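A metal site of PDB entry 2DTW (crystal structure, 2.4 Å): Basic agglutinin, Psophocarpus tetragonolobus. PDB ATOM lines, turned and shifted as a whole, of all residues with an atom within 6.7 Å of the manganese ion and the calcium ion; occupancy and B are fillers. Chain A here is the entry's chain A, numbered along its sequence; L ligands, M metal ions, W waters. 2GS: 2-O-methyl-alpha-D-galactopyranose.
O3 of the ligand sits at hydrogen-bond distance from OD2 of Asp 87, at 2.7 Å.
The backbone NH of Gly 105 is in hydrogen-bond range of an oxygen (O3) of the ligand, at 3.0 Å.
ND2 of Asn 128 is in hydrogen-bond range of O3 of the ligand (3.2 Å).
O of Asp 87 sits at hydrogen-bond distance from N of Phe 126 (3.5 Å).
The side-chain carboxylate (OD2) of Asp 140 sits close to the side-chain carboxylate (OE1) of Glu 122, 2.7 Å away.
NE1 of Trp 130 lies close to OD1 of Asp 131 (3.3 Å).
The backbone NH (N) of Glu 122 sits at hydrogen-bond distance from the backbone carbonyl oxygen (O) of Gly 138 (2.9 Å).
The backbone carbonyl oxygen of Asp 131 lies within hydrogen-bond range of the guanidinium group of Arg 127 (3.0 Å).
Within 4 Å of the manganese ion: Glu 122, Asp 124, Asp 131 and His 136.
The nearest printed residue that does not touch the manganese ion is Ser 146 (4.4 Å).
Four residues have an atom within 4 Å of the calcium ion: Asp 124, Phe 126, Asn 128 and Asp 131.
The manganese ion is bound by OD1 of Asp 131 (2.2 Å).
OE2 of Glu 122 binds the manganese ion (2.3 Å).
Water W2 binds the manganese ion (2.3 Å).
The manganese ion is bound by water W3, 2.3 Å away.
OD2 of Asp 124 binds the manganese ion (2.3 Å).
The manganese ion is bound by a ring nitrogen (NE2) of His 136 (2.3 Å).
The calcium ion is bound by OD2 of Asp 131, water W4, water W1, O of Phe 126, OD2 of Asp 124, OD1 of Asp 124 and OD1 of Asn 128.
The calcium ion has seven donor atoms within binding distance.
Water W2 lies within hydrogen-bond range of OE1 of Glu 122, O of Val 144 and NE1 of Trp 130.
Water W1 bridges O of Gly 105 and NE1 of Trp 130.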
ATOM      1  N   ASP A  87     -16.711  21.739  24.004  1.00  0.00           N
ATOM      2  CA  ASP A  87     -15.529  21.932  24.847  1.00  0.00           C
ATOM      3  C   ASP A  87     -14.623  23.050  24.310  1.00  0.00           C
ATOM      4  O   ASP A  87     -13.890  23.672  25.066  1.00  0.00           O
ATOM      5  CB  ASP A  87     -14.708  20.639  24.932  1.00  0.00           C
ATOM      6  CG  ASP A  87     -15.188  19.733  26.033  1.00  0.00           C
ATOM      7  OD1 ASP A  87     -16.092  18.901  25.770  1.00  0.00           O
ATOM      8  OD2 ASP A  87     -14.673  19.871  27.168  1.00  0.00           O
ATOM      9  N   GLY A 104     -13.702  15.505  24.350  1.00  0.00           N
ATOM     10  CA  GLY A 104     -13.855  16.330  25.532  1.00  0.00           C
ATOM     11  C   GLY A 104     -12.784  17.390  25.676  1.00  0.00           C
ATOM     12  O   GLY A 104     -12.399  18.044  24.693  1.00  0.00           O
ATOM     13  N   GLY A 105     -12.284  17.570  26.896  1.00  0.00           N
ATOM     14  CA  GLY A 105     -11.248  18.564  27.147  1.00  0.00           C
ATOM     15  C   GLY A 105      -9.936  18.365  26.416  1.00  0.00           C
ATOM     16  O   GLY A 105      -9.067  19.226  26.489  1.00  0.00           O
ATOM     17  N   TYR A 106      -9.788  17.246  25.717  1.00  0.00           N
ATOM     18  CA  TYR A 106      -8.569  16.990  24.966  1.00  0.00           C
ATOM     19  C   TYR A 106      -8.684  17.455  23.502  1.00  0.00           C
ATOM     20  O   TYR A 106      -7.739  17.322  22.716  1.00  0.00           O
ATOM     21  CB  TYR A 106      -8.218  15.506  25.039  1.00  0.00           C
ATOM     22  CG  TYR A 106      -7.870  15.077  26.445  1.00  0.00           C
ATOM     23  CD1 TYR A 106      -6.730  15.558  27.081  1.00  0.00           C
ATOM     24  CD2 TYR A 106      -8.712  14.227  27.171  1.00  0.00           C
ATOM     25  CE1 TYR A 106      -6.434  15.216  28.399  1.00  0.00           C
ATOM     26  CE2 TYR A 106      -8.429  13.884  28.484  1.00  0.00           C
ATOM     27  CZ  TYR A 106      -7.287  14.376  29.092  1.00  0.00           C
ATOM     28  OH  TYR A 106      -7.012  14.044  30.405  1.00  0.00           O
ATOM     29  N   PHE A 107      -9.858  17.990  23.172  1.00  0.00           N
ATOM     30  CA  PHE A 107     -10.118  18.553  21.852  1.00  0.00           C
ATOM     31  C   PHE A 107      -9.910  17.636  20.655  1.00  0.00           C
ATOM     32  O   PHE A 107     -10.067  18.071  19.518  1.00  0.00           O
ATOM     33  CB  PHE A 107      -9.245  19.794  21.654  1.00  0.00           C
ATOM     34  CG  PHE A 107      -9.400  20.829  22.741  1.00  0.00           C
ATOM     35  CD1 PHE A 107     -10.603  21.489  22.931  1.00  0.00           C
ATOM     36  CD2 PHE A 107      -8.318  21.160  23.546  1.00  0.00           C
ATOM     37  CE1 PHE A 107     -10.737  22.478  23.921  1.00  0.00           C
ATOM     38  CE2 PHE A 107      -8.430  22.140  24.541  1.00  0.00           C
ATOM     39  CZ  PHE A 107      -9.633  22.809  24.728  1.00  0.00           C
ATOM     40  N   GLU A 122      -5.665  27.133  21.732  1.00  0.00           N
ATOM     41  CA  GLU A 122      -7.010  26.710  22.062  1.00  0.00           C
ATOM     42  C   GLU A 122      -7.936  27.857  22.419  1.00  0.00           C
ATOM     43  O   GLU A 122      -7.523  28.897  22.920  1.00  0.00           O
ATOM     44  CB  GLU A 122      -6.986  25.747  23.258  1.00  0.00           C
ATOM     45  CG  GLU A 122      -6.437  26.386  24.514  1.00  0.00           C
ATOM     46  CD  GLU A 122      -6.659  25.559  25.772  1.00  0.00           C
ATOM     47  OE1 GLU A 122      -6.307  24.360  25.779  1.00  0.00           O
ATOM     48  OE2 GLU A 122      -7.171  26.132  26.753  1.00  0.00           O
ATOM     49  N   ASP A 124     -10.800  27.531  24.537  1.00  0.00           N
ATOM     50  CA  ASP A 124     -11.424  26.674  25.525  1.00  0.00           C
ATOM     51  C   ASP A 124     -12.714  27.230  26.099  1.00  0.00           C
ATOM     52  O   ASP A 124     -12.719  28.302  26.682  1.00  0.00           O
ATOM     53  CB  ASP A 124     -10.427  26.457  26.661  1.00  0.00           C
ATOM     54  CG  ASP A 124     -10.676  25.133  27.334  1.00  0.00           C
ATOM     55  OD1 ASP A 124     -11.538  24.339  26.855  1.00  0.00           O
ATOM     56  OD2 ASP A 124     -10.012  24.885  28.354  1.00  0.00           O
ATOM     57  N   THR A 125     -13.799  26.468  25.984  1.00  0.00           N
ATOM     58  CA  THR A 125     -15.093  26.912  26.484  1.00  0.00           C
ATOM     59  C   THR A 125     -15.583  26.178  27.736  1.00  0.00           C
ATOM     60  O   THR A 125     -16.546  26.607  28.370  1.00  0.00           O
ATOM     61  CB  THR A 125     -16.141  26.768  25.403  1.00  0.00           C
ATOM     62  OG1 THR A 125     -16.071  25.456  24.840  1.00  0.00           O
ATOM     63  CG2 THR A 125     -15.916  27.822  24.307  1.00  0.00           C
ATOM     64  N   PHE A 126     -14.927  25.066  28.072  1.00  0.00           N
ATOM     65  CA  PHE A 126     -15.326  24.288  29.242  1.00  0.00           C
ATOM     66  C   PHE A 126     -14.189  24.214  30.256  1.00  0.00           C
ATOM     67  O   PHE A 126     -13.044  23.901  29.902  1.00  0.00           O
ATOM     68  CB  PHE A 126     -15.730  22.871  28.846  1.00  0.00           C
ATOM     69  CG  PHE A 126     -16.067  22.007  30.018  1.00  0.00           C
ATOM     70  CD1 PHE A 126     -17.316  22.068  30.608  1.00  0.00           C
ATOM     71  CD2 PHE A 126     -15.090  21.180  30.583  1.00  0.00           C
ATOM     72  CE1 PHE A 126     -17.606  21.324  31.764  1.00  0.00           C
ATOM     73  CE2 PHE A 126     -15.357  20.446  31.737  1.00  0.00           C
ATOM     74  CZ  PHE A 126     -16.619  20.515  32.318  1.00  0.00           C
ATOM     75  N   ARG A 127     -14.509  24.456  31.518  1.00  0.00           N
ATOM     76  CA  ARG A 127     -13.477  24.434  32.549  1.00  0.00           C
ATOM     77  C   ARG A 127     -13.200  23.065  33.142  1.00  0.00           C
ATOM     78  O   ARG A 127     -13.924  22.592  34.006  1.00  0.00           O
ATOM     79  CB  ARG A 127     -13.822  25.414  33.670  1.00  0.00           C
ATOM     80  CG  ARG A 127     -12.697  25.558  34.670  1.00  0.00           C
ATOM     81  CD  ARG A 127     -12.960  26.624  35.714  1.00  0.00           C
ATOM     82  NE  ARG A 127     -11.740  26.941  36.463  1.00  0.00           N
ATOM     83  CZ  ARG A 127     -11.668  27.834  37.441  1.00  0.00           C
ATOM     84  NH1 ARG A 127     -12.754  28.494  37.820  1.00  0.00           N
ATOM     85  NH2 ARG A 127     -10.499  28.074  38.033  1.00  0.00           N
ATOM     86  N   ASN A 128     -12.120  22.437  32.674  1.00  0.00           N
ATOM     87  CA  ASN A 128     -11.703  21.137  33.204  1.00  0.00           C
ATOM     88  C   ASN A 128     -10.959  21.396  34.517  1.00  0.00           C
ATOM     89  O   ASN A 128     -10.738  22.545  34.893  1.00  0.00           O
ATOM     90  CB  ASN A 128     -10.770  20.433  32.220  1.00  0.00           C
ATOM     91  CG  ASN A 128     -11.481  19.688  31.095  1.00  0.00           C
ATOM     92  OD1 ASN A 128     -11.535  20.152  29.959  1.00  0.00           O
ATOM     93  ND2 ASN A 128     -12.031  18.516  31.424  1.00  0.00           N
ATOM     94  N   TRP A 130      -7.909  21.170  35.159  1.00  0.00           N
ATOM     95  CA  TRP A 130      -6.634  21.827  34.882  1.00  0.00           C
ATOM     96  C   TRP A 130      -6.789  23.222  34.284  1.00  0.00           C
ATOM     97  O   TRP A 130      -5.782  23.871  33.990  1.00  0.00           O
ATOM     98  CB  TRP A 130      -5.828  20.964  33.918  1.00  0.00           C
ATOM     99  CG  TRP A 130      -6.554  20.747  32.605  1.00  0.00           C
ATOM    100  CD1 TRP A 130      -6.741  21.657  31.603  1.00  0.00           C
ATOM    101  CD2 TRP A 130      -7.215  19.550  32.177  1.00  0.00           C
ATOM    102  NE1 TRP A 130      -7.477  21.110  30.582  1.00  0.00           N
ATOM    103  CE2 TRP A 130      -7.776  19.813  30.912  1.00  0.00           C
ATOM    104  CE3 TRP A 130      -7.389  18.271  32.744  1.00  0.00           C
ATOM    105  CZ2 TRP A 130      -8.509  18.854  30.193  1.00  0.00           C
ATOM    106  CZ3 TRP A 130      -8.118  17.315  32.033  1.00  0.00           C
ATOM    107  CH2 TRP A 130      -8.661  17.610  30.772  1.00  0.00           C
ATOM    108  N   ASP A 131      -8.029  23.684  34.099  1.00  0.00           N
ATOM    109  CA  ASP A 131      -8.305  24.981  33.485  1.00  0.00           C
ATOM    110  C   ASP A 131      -8.580  26.158  34.392  1.00  0.00           C
ATOM    111  O   ASP A 131      -9.079  26.001  35.506  1.00  0.00           O
ATOM    112  CB  ASP A 131      -9.534  24.933  32.566  1.00  0.00           C
ATOM    113  CG  ASP A 131      -9.353  24.223  31.263  1.00  0.00           C
ATOM    114  OD1 ASP A 131      -8.256  24.320  30.686  1.00  0.00           O
ATOM    115  OD2 ASP A 131     -10.341  23.590  30.808  1.00  0.00           O
ATOM    116  N   PRO A 132      -8.261  27.371  33.922  1.00  0.00           N
ATOM    117  CA  PRO A 132      -8.508  28.591  34.687  1.00  0.00           C
ATOM    118  C   PRO A 132      -9.913  28.977  34.189  1.00  0.00           C
ATOM    119  O   PRO A 132     -10.538  28.196  33.475  1.00  0.00           O
ATOM    120  CB  PRO A 132      -7.438  29.540  34.170  1.00  0.00           C
ATOM    121  CG  PRO A 132      -7.322  29.135  32.733  1.00  0.00           C
ATOM    122  CD  PRO A 132      -7.302  27.619  32.836  1.00  0.00           C
ATOM    123  N   ILE A 134     -13.139  30.182  32.207  1.00  0.00           N
ATOM    124  CA  ILE A 134     -13.431  30.083  30.787  1.00  0.00           C
ATOM    125  C   ILE A 134     -14.465  31.151  30.416  1.00  0.00           C
ATOM    126  O   ILE A 134     -15.210  31.628  31.258  1.00  0.00           O
ATOM    127  CB  ILE A 134     -13.925  28.656  30.387  1.00  0.00           C
ATOM    128  CG1 ILE A 134     -15.119  28.238  31.246  1.00  0.00           C
ATOM    129  CG2 ILE A 134     -12.785  27.659  30.492  1.00  0.00           C
ATOM    130  CD1 ILE A 134     -16.458  28.887  30.834  1.00  0.00           C
ATOM    131  N   HIS A 136     -11.267  30.975  27.555  1.00  0.00           N
ATOM    132  CA  HIS A 136      -9.922  31.513  27.541  1.00  0.00           C
ATOM    133  C   HIS A 136      -9.142  31.033  26.340  1.00  0.00           C
ATOM    134  O   HIS A 136      -9.429  29.987  25.774  1.00  0.00           O
ATOM    135  CB  HIS A 136      -9.152  31.155  28.827  1.00  0.00           C
ATOM    136  CG  HIS A 136      -9.014  29.696  29.099  1.00  0.00           C
ATOM    137  ND1 HIS A 136      -9.891  28.999  29.891  1.00  0.00           N
ATOM    138  CD2 HIS A 136      -8.067  28.794  28.717  1.00  0.00           C
ATOM    139  CE1 HIS A 136      -9.502  27.737  29.995  1.00  0.00           C
ATOM    140  NE2 HIS A 136      -8.398  27.597  29.290  1.00  0.00           N
ATOM    141  N   ILE A 137      -8.175  31.843  25.928  1.00  0.00           N
ATOM    142  CA  ILE A 137      -7.303  31.483  24.829  1.00  0.00           C
ATOM    143  C   ILE A 137      -6.107  30.869  25.532  1.00  0.00           C
ATOM    144  O   ILE A 137      -5.721  31.332  26.612  1.00  0.00           O
ATOM    145  CB  ILE A 137      -6.806  32.700  24.060  1.00  0.00           C
ATOM    146  CG1 ILE A 137      -7.975  33.533  23.555  1.00  0.00           C
ATOM    147  CG2 ILE A 137      -5.965  32.242  22.893  1.00  0.00           C
ATOM    148  CD1 ILE A 137      -7.546  34.767  22.798  1.00  0.00           C
ATOM    149  N   GLY A 138      -5.541  29.834  24.952  1.00  0.00           N
ATOM    150  CA  GLY A 138      -4.393  29.218  25.586  1.00  0.00           C
ATOM    151  C   GLY A 138      -3.389  28.726  24.577  1.00  0.00           C
ATOM    152  O   GLY A 138      -3.739  28.384  23.451  1.00  0.00           O
ATOM    153  N   ASP A 140      -0.800  25.829  23.906  1.00  0.00           N
ATOM    154  CA  ASP A 140      -0.495  24.484  24.363  1.00  0.00           C
ATOM    155  C   ASP A 140       0.692  23.864  23.662  1.00  0.00           C
ATOM    156  O   ASP A 140       0.794  23.900  22.445  1.00  0.00           O
ATOM    157  CB  ASP A 140      -1.721  23.581  24.199  1.00  0.00           C
ATOM    158  CG  ASP A 140      -2.994  24.206  24.730  1.00  0.00           C
ATOM    159  OD1 ASP A 140      -2.920  25.176  25.508  1.00  0.00           O
ATOM    160  OD2 ASP A 140      -4.082  23.709  24.376  1.00  0.00           O
ATOM    161  N   VAL A 144      -2.511  19.799  27.147  1.00  0.00           N
ATOM    162  CA  VAL A 144      -3.655  20.700  27.158  1.00  0.00           C
ATOM    163  C   VAL A 144      -3.577  21.632  28.361  1.00  0.00           C
ATOM    164  O   VAL A 144      -4.458  22.471  28.575  1.00  0.00           O
ATOM    165  CB  VAL A 144      -4.989  19.889  27.182  1.00  0.00           C
ATOM    166  CG1 VAL A 144      -5.189  19.161  25.882  1.00  0.00           C
ATOM    167  CG2 VAL A 144      -4.933  18.871  28.314  1.00  0.00           C
ATOM    168  N   ILE A 145      -2.533  21.476  29.169  1.00  0.00           N
ATOM    169  CA  ILE A 145      -2.335  22.341  30.318  1.00  0.00           C
ATOM    170  C   ILE A 145      -1.474  23.486  29.792  1.00  0.00           C
ATOM    171  O   ILE A 145      -0.245  23.410  29.778  1.00  0.00           O
ATOM    172  CB  ILE A 145      -1.595  21.606  31.439  1.00  0.00           C
ATOM    173  CG1 ILE A 145      -2.462  20.438  31.930  1.00  0.00           C
ATOM    174  CG2 ILE A 145      -1.284  22.554  32.590  1.00  0.00           C
ATOM    175  CD1 ILE A 145      -1.761  19.563  32.956  1.00  0.00           C
ATOM    176  N   SER A 146      -2.144  24.533  29.335  1.00  0.00           N
ATOM    177  CA  SER A 146      -1.515  25.709  28.729  1.00  0.00           C
ATOM    178  C   SER A 146      -0.333  26.314  29.475  1.00  0.00           C
ATOM    179  O   SER A 146      -0.311  26.342  30.706  1.00  0.00           O
ATOM    180  CB  SER A 146      -2.561  26.803  28.515  1.00  0.00           C
ATOM    181  OG  SER A 146      -3.642  26.336  27.745  1.00  0.00           O
ATOM    182  N   THR A 149      -2.253  31.690  29.380  1.00  0.00           N
ATOM    183  CA  THR A 149      -3.689  31.773  29.219  1.00  0.00           C
ATOM    184  C   THR A 149      -4.213  33.195  29.371  1.00  0.00           C
ATOM    185  O   THR A 149      -3.645  34.002  30.125  1.00  0.00           O
ATOM    186  CB  THR A 149      -4.337  30.849  30.286  1.00  0.00           C
ATOM    187  OG1 THR A 149      -4.720  29.607  29.670  1.00  0.00           O
ATOM    188  CG2 THR A 149      -5.504  31.504  30.967  1.00  0.00           C
HETATM  189  C1  2GS L   1     -16.434  15.652  31.031  1.00  0.00           C
HETATM  190  C2  2GS L   1     -15.210  16.140  30.135  1.00  0.00           C
HETATM  191  C3  2GS L   1     -15.277  17.711  29.941  1.00  0.00           C
HETATM  192  C4  2GS L   1     -16.659  18.099  29.306  1.00  0.00           C
HETATM  193  C5  2GS L   1     -17.806  17.601  30.241  1.00  0.00           C
HETATM  194  C6  2GS L   1     -19.156  17.923  29.660  1.00  0.00           C
HETATM  195  C7  2GS L   1     -12.773  15.427  29.933  1.00  0.00           C
HETATM  196  O1  2GS L   1     -16.320  16.118  32.391  1.00  0.00           O
HETATM  197  O2  2GS L   1     -13.950  15.717  30.722  1.00  0.00           O
HETATM  198  O3  2GS L   1     -14.198  18.143  29.141  1.00  0.00           O
HETATM  199  O4  2GS L   1     -16.781  17.553  27.989  1.00  0.00           O
HETATM  200  O5  2GS L   1     -17.715  16.132  30.423  1.00  0.00           O
HETATM  201  O6  2GS L   1     -20.208  17.467  30.514  1.00  0.00           O
HETATM  202 MN    MN M   1      -7.826  25.398  28.789  1.00  0.00          MN
HETATM  203 CA    CA M   2     -11.218  22.759  28.811  1.00  0.00          CA
HETATM  204  O   HOH W   1      -9.280  21.667  27.872  1.00  0.00           O
HETATM  205  O   HOH W   2      -7.121  23.346  28.145  1.00  0.00           O
HETATM  206  O   HOH W   3      -5.701  25.988  29.341  1.00  0.00           O
HETATM  207  O   HOH W   4     -12.684  21.760  27.272  1.00  0.00           O
